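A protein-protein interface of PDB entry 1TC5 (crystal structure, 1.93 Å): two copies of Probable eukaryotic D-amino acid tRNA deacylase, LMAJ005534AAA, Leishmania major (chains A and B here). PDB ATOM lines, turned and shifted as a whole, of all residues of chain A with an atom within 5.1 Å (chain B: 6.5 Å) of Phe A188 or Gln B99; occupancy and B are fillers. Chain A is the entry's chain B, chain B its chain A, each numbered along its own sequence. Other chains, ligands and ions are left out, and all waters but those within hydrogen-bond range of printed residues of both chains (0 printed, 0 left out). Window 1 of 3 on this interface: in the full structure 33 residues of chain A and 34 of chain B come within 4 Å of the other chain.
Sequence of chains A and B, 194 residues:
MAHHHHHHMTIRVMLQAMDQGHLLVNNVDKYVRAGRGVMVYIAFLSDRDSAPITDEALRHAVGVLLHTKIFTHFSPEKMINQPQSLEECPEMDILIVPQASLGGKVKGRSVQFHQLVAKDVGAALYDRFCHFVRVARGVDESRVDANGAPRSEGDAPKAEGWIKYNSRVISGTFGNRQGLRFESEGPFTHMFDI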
ATOM      1  N   LEU A  15      20.806  25.224  17.645  1.00  0.00           N
ATOM      2  CA  LEU A  15      21.117  26.363  18.486  1.00  0.00           C
ATOM      3  C   LEU A  15      19.893  27.228  18.615  1.00  0.00           C
ATOM      4  O   LEU A  15      19.289  27.589  17.597  1.00  0.00           O
ATOM      5  CB  LEU A  15      22.231  27.197  17.838  1.00  0.00           C
ATOM      6  CG  LEU A  15      23.489  26.426  17.429  1.00  0.00           C
ATOM      7  CD1 LEU A  15      24.500  27.307  16.643  1.00  0.00           C
ATOM      8  CD2 LEU A  15      24.159  25.817  18.645  1.00  0.00           C
ATOM      9  N   ALA A  17      18.082  30.687  20.761  1.00  0.00           N
ATOM     10  CA  ALA A  17      18.167  31.857  21.628  1.00  0.00           C
ATOM     11  C   ALA A  17      17.467  31.573  22.961  1.00  0.00           C
ATOM     12  O   ALA A  17      16.248  31.374  23.027  1.00  0.00           O
ATOM     13  CB  ALA A  17      17.535  33.079  20.939  1.00  0.00           C
ATOM     14  N   ILE A  70      25.434  34.964  15.141  1.00  0.00           N
ATOM     15  CA  ILE A  70      24.182  34.263  14.877  1.00  0.00           C
ATOM     16  C   ILE A  70      22.992  34.997  15.450  1.00  0.00           C
ATOM     17  O   ILE A  70      22.075  35.364  14.725  1.00  0.00           O
ATOM     18  CB  ILE A  70      24.238  32.821  15.462  1.00  0.00           C
ATOM     19  CG1 ILE A  70      25.497  32.083  14.955  1.00  0.00           C
ATOM     20  CG2 ILE A  70      22.953  32.079  15.146  1.00  0.00           C
ATOM     21  CD1 ILE A  70      25.968  30.942  15.838  1.00  0.00           C
ATOM     22  N   PHE A  71      23.024  35.215  16.761  1.00  0.00           N
ATOM     23  CA  PHE A  71      21.860  35.680  17.504  1.00  0.00           C
ATOM     24  C   PHE A  71      21.803  37.193  17.755  1.00  0.00           C
ATOM     25  O   PHE A  71      22.827  37.871  17.842  1.00  0.00           O
ATOM     26  CB  PHE A  71      21.730  34.909  18.811  1.00  0.00           C
ATOM     27  CG  PHE A  71      21.552  33.430  18.623  1.00  0.00           C
ATOM     28  CD1 PHE A  71      20.364  32.925  18.154  1.00  0.00           C
ATOM     29  CD2 PHE A  71      22.617  32.542  18.860  1.00  0.00           C
ATOM     30  CE1 PHE A  71      20.206  31.562  17.935  1.00  0.00           C
ATOM     31  CE2 PHE A  71      22.449  31.185  18.672  1.00  0.00           C
ATOM     32  CZ  PHE A  71      21.234  30.706  18.210  1.00  0.00           C
ATOM     33  N   THR A  72      20.574  37.699  17.871  1.00  0.00           N
ATOM     34  CA  THR A  72      20.260  39.135  17.954  1.00  0.00           C
ATOM     35  C   THR A  72      19.704  39.573  19.327  1.00  0.00           C
ATOM     36  O   THR A  72      19.351  40.751  19.516  1.00  0.00           O
ATOM     37  CB  THR A  72      19.200  39.529  16.868  1.00  0.00           C
ATOM     38  OG1 THR A  72      18.027  38.718  16.998  1.00  0.00           O
ATOM     39  CG2 THR A  72      19.691  39.215  15.409  1.00  0.00           C
ATOM     40  N   GLY A 186      12.190  34.216  21.334  1.00  0.00           N
ATOM     41  CA  GLY A 186      12.161  33.920  19.906  1.00  0.00           C
ATOM     42  C   GLY A 186      13.367  33.057  19.622  1.00  0.00           C
ATOM     43  O   GLY A 186      14.475  33.595  19.579  1.00  0.00           O
ATOM     44  N   PRO A 187      13.194  31.733  19.533  1.00  0.00           N
ATOM     45  CA  PRO A 187      14.344  30.821  19.479  1.00  0.00           C
ATOM     46  C   PRO A 187      15.270  31.044  18.318  1.00  0.00           C
ATOM     47  O   PRO A 187      16.458  30.723  18.487  1.00  0.00           O
ATOM     48  CB  PRO A 187      13.716  29.417  19.393  1.00  0.00           C
ATOM     49  CG  PRO A 187      12.277  29.583  19.896  1.00  0.00           C
ATOM     50  CD  PRO A 187      11.909  31.002  19.532  1.00  0.00           C
ATOM     51  N   PHE A 188      14.782  31.542  17.177  1.00  0.00           N
ATOM     52  CA  PHE A 188      15.663  31.830  16.024  1.00  0.00           C
ATOM     53  C   PHE A 188      16.596  30.657  15.737  1.00  0.00           C
ATOM     54  O   PHE A 188      17.812  30.810  15.578  1.00  0.00           O
ATOM     55  CB  PHE A 188      16.470  33.088  16.334  1.00  0.00           C
ATOM     56  CG  PHE A 188      17.130  33.749  15.151  1.00  0.00           C
ATOM     57  CD1 PHE A 188      16.675  33.591  13.846  1.00  0.00           C
ATOM     58  CD2 PHE A 188      18.236  34.586  15.376  1.00  0.00           C
ATOM     59  CE1 PHE A 188      17.285  34.230  12.806  1.00  0.00           C
ATOM     60  CE2 PHE A 188      18.849  35.236  14.336  1.00  0.00           C
ATOM     61  CZ  PHE A 188      18.370  35.053  13.030  1.00  0.00           C
ATOM     62  N   THR A 189      15.997  29.485  15.647  1.00  0.00           N
ATOM     63  CA  THR A 189      16.718  28.231  15.672  1.00  0.00           C
ATOM     64  C   THR A 189      17.589  28.070  14.452  1.00  0.00           C
ATOM     65  O   THR A 189      17.143  28.312  13.330  1.00  0.00           O
ATOM     66  CB  THR A 189      15.737  27.046  15.805  1.00  0.00           C
ATOM     67  OG1 THR A 189      14.941  27.241  16.979  1.00  0.00           O
ATOM     68  CG2 THR A 189      16.484  25.717  16.075  1.00  0.00           C
ATOM     69  N   HIS A 190      18.852  27.739  14.703  1.00  0.00           N
ATOM     70  CA  HIS A 190      19.768  27.353  13.659  1.00  0.00           C
ATOM     71  C   HIS A 190      20.122  25.870  13.825  1.00  0.00           C
ATOM     72  O   HIS A 190      20.046  25.301  14.934  1.00  0.00           O
ATOM     73  CB  HIS A 190      21.033  28.229  13.666  1.00  0.00           C
ATOM     74  CG  HIS A 190      20.776  29.667  13.302  1.00  0.00           C
ATOM     75  ND1 HIS A 190      20.044  30.517  14.103  1.00  0.00           N
ATOM     76  CD2 HIS A 190      21.143  30.396  12.221  1.00  0.00           C
ATOM     77  CE1 HIS A 190      20.004  31.719  13.549  1.00  0.00           C
ATOM     78  NE2 HIS A 190      20.661  31.671  12.402  1.00  0.00           N
ATOM     79  N   ARG B  12      12.284  21.039   6.075  1.00  0.00           N
ATOM     80  CA  ARG B  12      13.080  20.679   7.253  1.00  0.00           C
ATOM     81  C   ARG B  12      12.244  20.840   8.501  1.00  0.00           C
ATOM     82  O   ARG B  12      11.671  21.902   8.728  1.00  0.00           O
ATOM     83  CB  ARG B  12      14.298  21.600   7.363  1.00  0.00           C
ATOM     84  CG  ARG B  12      15.134  21.404   8.641  1.00  0.00           C
ATOM     85  CD  ARG B  12      16.542  21.918   8.510  1.00  0.00           C
ATOM     86  NE  ARG B  12      17.256  21.146   7.494  1.00  0.00           N
ATOM     87  CZ  ARG B  12      18.364  21.548   6.876  1.00  0.00           C
ATOM     88  NH1 ARG B  12      18.938  22.689   7.179  1.00  0.00           N
ATOM     89  NH2 ARG B  12      18.910  20.783   5.959  1.00  0.00           N
ATOM     90  N   VAL B  40       6.820  21.174  16.766  1.00  0.00           N
ATOM     91  CA  VAL B  40       7.383  21.094  15.426  1.00  0.00           C
ATOM     92  C   VAL B  40       7.917  22.468  15.069  1.00  0.00           C
ATOM     93  O   VAL B  40       7.148  23.427  15.080  1.00  0.00           O
ATOM     94  CB  VAL B  40       6.267  20.726  14.407  1.00  0.00           C
ATOM     95  CG1 VAL B  40       6.785  20.679  12.979  1.00  0.00           C
ATOM     96  CG2 VAL B  40       5.594  19.403  14.777  1.00  0.00           C
ATOM     97  N   TYR B  41       9.212  22.564  14.782  1.00  0.00           N
ATOM     98  CA  TYR B  41       9.807  23.714  14.108  1.00  0.00           C
ATOM     99  C   TYR B  41       9.935  23.416  12.603  1.00  0.00           C
ATOM    100  O   TYR B  41      10.441  22.379  12.225  1.00  0.00           O
ATOM    101  CB  TYR B  41      11.203  24.000  14.655  1.00  0.00           C
ATOM    102  CG  TYR B  41      11.358  24.480  16.086  1.00  0.00           C
ATOM    103  CD1 TYR B  41      10.279  24.767  16.888  1.00  0.00           C
ATOM    104  CD2 TYR B  41      12.639  24.653  16.636  1.00  0.00           C
ATOM    105  CE1 TYR B  41      10.454  25.205  18.217  1.00  0.00           C
ATOM    106  CE2 TYR B  41      12.823  25.089  17.935  1.00  0.00           C
ATOM    107  CZ  TYR B  41      11.724  25.373  18.731  1.00  0.00           C
ATOM    108  OH  TYR B  41      11.889  25.809  20.038  1.00  0.00           O
ATOM    109  N   ILE B  42       9.512  24.340  11.740  1.00  0.00           N
ATOM    110  CA  ILE B  42       9.474  24.060  10.321  1.00  0.00           C
ATOM    111  C   ILE B  42      10.084  25.175   9.450  1.00  0.00           C
ATOM    112  O   ILE B  42       9.864  26.364   9.664  1.00  0.00           O
ATOM    113  CB  ILE B  42       7.992  23.746   9.890  1.00  0.00           C
ATOM    114  CG1 ILE B  42       7.907  23.278   8.437  1.00  0.00           C
ATOM    115  CG2 ILE B  42       7.054  24.926  10.163  1.00  0.00           C
ATOM    116  CD1 ILE B  42       6.600  22.512   8.179  1.00  0.00           C
ATOM    117  N   ALA B  43      10.815  24.746   8.437  1.00  0.00           N
ATOM    118  CA  ALA B  43      11.419  25.629   7.450  1.00  0.00           C
ATOM    119  C   ALA B  43      11.248  24.992   6.096  1.00  0.00           C
ATOM    120  O   ALA B  43      11.296  23.768   5.971  1.00  0.00           O
ATOM    121  CB  ALA B  43      12.879  25.788   7.719  1.00  0.00           C
ATOM    122  N   PHE B  44      11.067  25.845   5.096  1.00  0.00           N
ATOM    123  CA  PHE B  44      10.884  25.455   3.730  1.00  0.00           C
ATOM    124  C   PHE B  44      12.073  25.979   2.949  1.00  0.00           C
ATOM    125  O   PHE B  44      12.279  27.183   2.854  1.00  0.00           O
ATOM    126  CB  PHE B  44       9.543  25.994   3.165  1.00  0.00           C
ATOM    127  CG  PHE B  44       8.344  25.526   3.938  1.00  0.00           C
ATOM    128  CD1 PHE B  44       7.832  24.261   3.743  1.00  0.00           C
ATOM    129  CD2 PHE B  44       7.731  26.347   4.857  1.00  0.00           C
ATOM    130  CE1 PHE B  44       6.744  23.812   4.463  1.00  0.00           C
ATOM    131  CE2 PHE B  44       6.644  25.893   5.591  1.00  0.00           C
ATOM    132  CZ  PHE B  44       6.159  24.627   5.396  1.00  0.00           C
ATOM    133  N   VAL B  97       5.737  25.746  15.042  1.00  0.00           N
ATOM    134  CA  VAL B  97       6.406  27.024  15.044  1.00  0.00           C
ATOM    135  C   VAL B  97       7.206  27.212  13.743  1.00  0.00           C
ATOM    136  O   VAL B  97       8.090  26.401  13.432  1.00  0.00           O
ATOM    137  CB  VAL B  97       7.360  27.109  16.241  1.00  0.00           C
ATOM    138  CG1 VAL B  97       7.884  28.508  16.425  1.00  0.00           C
ATOM    139  CG2 VAL B  97       6.644  26.605  17.502  1.00  0.00           C
ATOM    140  N   PRO B  98       6.947  28.296  13.014  1.00  0.00           N
ATOM    141  CA  PRO B  98       7.739  28.582  11.824  1.00  0.00           C
ATOM    142  C   PRO B  98       9.133  29.009  12.273  1.00  0.00           C
ATOM    143  O   PRO B  98       9.261  29.906  13.111  1.00  0.00           O
ATOM    144  CB  PRO B  98       6.975  29.733  11.146  1.00  0.00           C
ATOM    145  CG  PRO B  98       6.211  30.420  12.245  1.00  0.00           C
ATOM    146  CD  PRO B  98       5.951  29.359  13.287  1.00  0.00           C
ATOM    147  N   GLN B  99      10.152  28.326  11.754  1.00  0.00           N
ATOM    148  CA  GLN B  99      11.544  28.611  12.078  1.00  0.00           C
ATOM    149  C   GLN B  99      12.378  28.491  10.818  1.00  0.00           C
ATOM    150  O   GLN B  99      13.099  27.527  10.653  1.00  0.00           O
ATOM    151  CB  GLN B  99      12.033  27.629  13.138  1.00  0.00           C
ATOM    152  CG  GLN B  99      11.407  27.850  14.496  1.00  0.00           C
ATOM    153  CD  GLN B  99      12.035  29.025  15.216  1.00  0.00           C
ATOM    154  OE1 GLN B  99      13.125  28.878  15.781  1.00  0.00           O
ATOM    155  NE2 GLN B  99      11.377  30.203  15.166  1.00  0.00           N
ATOM    156  N   ALA B 100      12.278  29.507   9.962  1.00  0.00           N
ATOM    157  CA  ALA B 100      12.903  29.524   8.653  1.00  0.00           C
ATOM    158  C   ALA B 100      14.426  29.497   8.784  1.00  0.00           C
ATOM    159  O   ALA B 100      15.117  29.005   7.891  1.00  0.00           O
ATOM    160  CB  ALA B 100      12.447  30.760   7.886  1.00  0.00           C
ATOM    161  N   SER B 101      14.917  29.982   9.925  1.00  0.00           N
ATOM    162  CA  SER B 101      16.354  30.067  10.219  1.00  0.00           C
ATOM    163  C   SER B 101      17.074  28.712  10.285  1.00  0.00           C
ATOM    164  O   SER B 101      18.309  28.667  10.265  1.00  0.00           O
ATOM    165  CB  SER B 101      16.547  30.801  11.538  1.00  0.00           C
ATOM    166  OG  SER B 101      15.715  30.260  12.561  1.00  0.00           O
ATOM    167  N   LEU B 102      16.307  27.622  10.356  1.00  0.00           N
ATOM    168  CA  LEU B 102      16.816  26.233  10.226  1.00  0.00           C
ATOM    169  C   LEU B 102      17.576  25.965   8.914  1.00  0.00           C
ATOM    170  O   LEU B 102      18.378  25.012   8.837  1.00  0.00           O
ATOM    171  CB  LEU B 102      15.646  25.224  10.293  1.00  0.00           C
ATOM    172  CG  LEU B 102      14.958  25.021  11.652  1.00  0.00           C
ATOM    173  CD1 LEU B 102      13.652  24.226  11.491  1.00  0.00           C
ATOM    174  CD2 LEU B 102      15.911  24.340  12.653  1.00  0.00           C
ATOM    175  N   GLY B 103      17.309  26.795   7.895  1.00  0.00           N
ATOM    176  CA  GLY B 103      18.012  26.729   6.619  1.00  0.00           C
ATOM    177  C   GLY B 103      19.283  27.552   6.557  1.00  0.00           C
ATOM    178  O   GLY B 103      20.002  27.472   5.569  1.00  0.00           O
ATOM    179  N   PHE B 113      21.306  32.896   4.503  1.00  0.00           N
ATOM    180  CA  PHE B 113      19.980  32.302   4.432  1.00  0.00           C
ATOM    181  C   PHE B 113      19.521  32.060   2.981  1.00  0.00           C
ATOM    182  O   PHE B 113      18.319  32.022   2.675  1.00  0.00           O
ATOM    183  CB  PHE B 113      18.991  33.208   5.163  1.00  0.00           C
ATOM    184  CG  PHE B 113      19.207  33.248   6.679  1.00  0.00           C
ATOM    185  CD1 PHE B 113      18.954  32.105   7.469  1.00  0.00           C
ATOM    186  CD2 PHE B 113      19.632  34.418   7.300  1.00  0.00           C
ATOM    187  CE1 PHE B 113      19.125  32.137   8.842  1.00  0.00           C
ATOM    188  CE2 PHE B 113      19.826  34.470   8.716  1.00  0.00           C
ATOM    189  CZ  PHE B 113      19.582  33.329   9.480  1.00  0.00           C
ATOM    190  N   TYR B 126       3.428  27.356   4.570  1.00  0.00           N
ATOM    191  CA  TYR B 126       3.246  27.228   6.022  1.00  0.00           C
ATOM    192  C   TYR B 126       1.769  27.134   6.367  1.00  0.00           C
ATOM    193  O   TYR B 126       1.337  26.284   7.155  1.00  0.00           O
ATOM    194  CB  TYR B 126       3.817  28.436   6.760  1.00  0.00           C
ATOM    195  CG  TYR B 126       3.533  28.432   8.245  1.00  0.00           C
ATOM    196  CD1 TYR B 126       4.163  27.517   9.090  1.00  0.00           C
ATOM    197  CD2 TYR B 126       2.646  29.330   8.806  1.00  0.00           C
ATOM    198  CE1 TYR B 126       3.893  27.481  10.452  1.00  0.00           C
ATOM    199  CE2 TYR B 126       2.386  29.310  10.168  1.00  0.00           C
ATOM    200  CZ  TYR B 126       3.011  28.389  10.987  1.00  0.00           C
ATOM    201  OH  TYR B 126       2.762  28.379  12.356  1.00  0.00           O
ATOM    202  N   GLN B 178       8.452  34.481  17.731  1.00  0.00           N
ATOM    203  CA  GLN B 178       7.875  33.252  18.299  1.00  0.00           C
ATOM    204  C   GLN B 178       8.315  33.072  19.769  1.00  0.00           C
ATOM    205  O   GLN B 178       9.052  32.125  20.141  1.00  0.00           O
ATOM    206  CB  GLN B 178       8.274  32.049  17.440  1.00  0.00           C
ATOM    207  CG  GLN B 178       7.976  32.189  15.940  1.00  0.00           C
ATOM    208  CD  GLN B 178       6.493  32.319  15.647  1.00  0.00           C
ATOM    209  OE1 GLN B 178       5.662  31.589  16.218  1.00  0.00           O
ATOM    210  NE2 GLN B 178       6.150  33.265  14.782  1.00  0.00           N
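The backbone carbonyl oxygen of Thr A189 is in hydrogen-bond range of the side-chain hydroxyl of Ser B101 (2.5 Å). The side-chain amide oxygen of Gln B99 lies within hydrogen-bond range of the backbone NH of Phe A188, 3.4 Å away. The backbone carbonyl oxygen (O) of Thr A189 lies within hydrogen-bond range of the backbone NH (N) of Leu B102, at 3.2 Å. The side-chain amide oxygen (OE1) of Gln B99 sits at hydrogen-bond distance from the side-chain hydroxyl (OG1) of Thr A189.
The backbone carbonyl oxygen of Phe A188 is in hydrogen-bond range of a ring nitrogen (ND1) of His A190, at 2.7 Å. N of Leu A15 sits at hydrogen-bond distance from O of His A190 (2.8 Å). The backbone carbonyl oxygen of Ile B42 lies within hydrogen-bond range of the backbone NH of Gln B99 (2.9 Å). N of Ala A17 sits at hydrogen-bond distance from O of Pro A187 (2.8 Å). The guanidinium group (NH1) of Arg B12 sits at hydrogen-bond distance from the backbone carbonyl oxygen (O) of Leu B102 (2.9 Å).
Gln B178 touches Gly A186. OH of Tyr B41 touches CG of Pro A187 (3.8 Å). CB of Pro A187 touches OE1 of Gln B99 (3.7 Å). Gln B178 touches Pro A187. Phe A188 touches Ser B101 (C to OG, 3.3 Å). CE2 of Tyr B41 touches OG1 of Thr A189, 3.2 Å away. His A190 touches Ser B101. His A190 touches Phe B113.
Of the printed residues of chain B, Phe A188 touches Gln B99 (3.4 Å) and Ser B101 (3.3 Å). Of chain A, only Pro A187 (3.7 Å), Phe A188 (3.4 Å) and Thr A189 (2.7 Å) come within 4 Å of Gln B99. Of the printed residues of chain B, Gly A186 touches Gln B178. Of the printed residues of chain B, Thr A189 touches Tyr B41 (3.2 Å), Gln B99 (2.7 Å), Ser B101 (2.5 Å) and Leu B102 (3.2 Å). Ala B43 touches none of the printed residues of chain A. Leu A15 touches none of the printed residues of chain B. The nearest residue of chain B that does not touch Phe A188 is Phe B113 (4.1 Å).
Of the 10 printed residues of chain A, 5 touch a printed residue of chain B. Hydrophobic or aromatic side chains of chain A within 4 Å of the printed part of chain B: Pro A187, Phe A188 and His A190. Of the 16 printed residues of chain B, 6 touch a printed residue of chain A. Hydrophobic or aromatic side chains of chain B that line the printed part of chain A: Tyr B41, Leu B102 and Phe B113. Among the printed residues, no Asp or Glu carboxylate lies within 4 Å of a Lys or Arg side-chain nitrogen of the other chain.
No position is printed for both chains. Of the 12 pairs that touch across the chains among the printed residues, none has its exchanged pair printed and touching as well.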
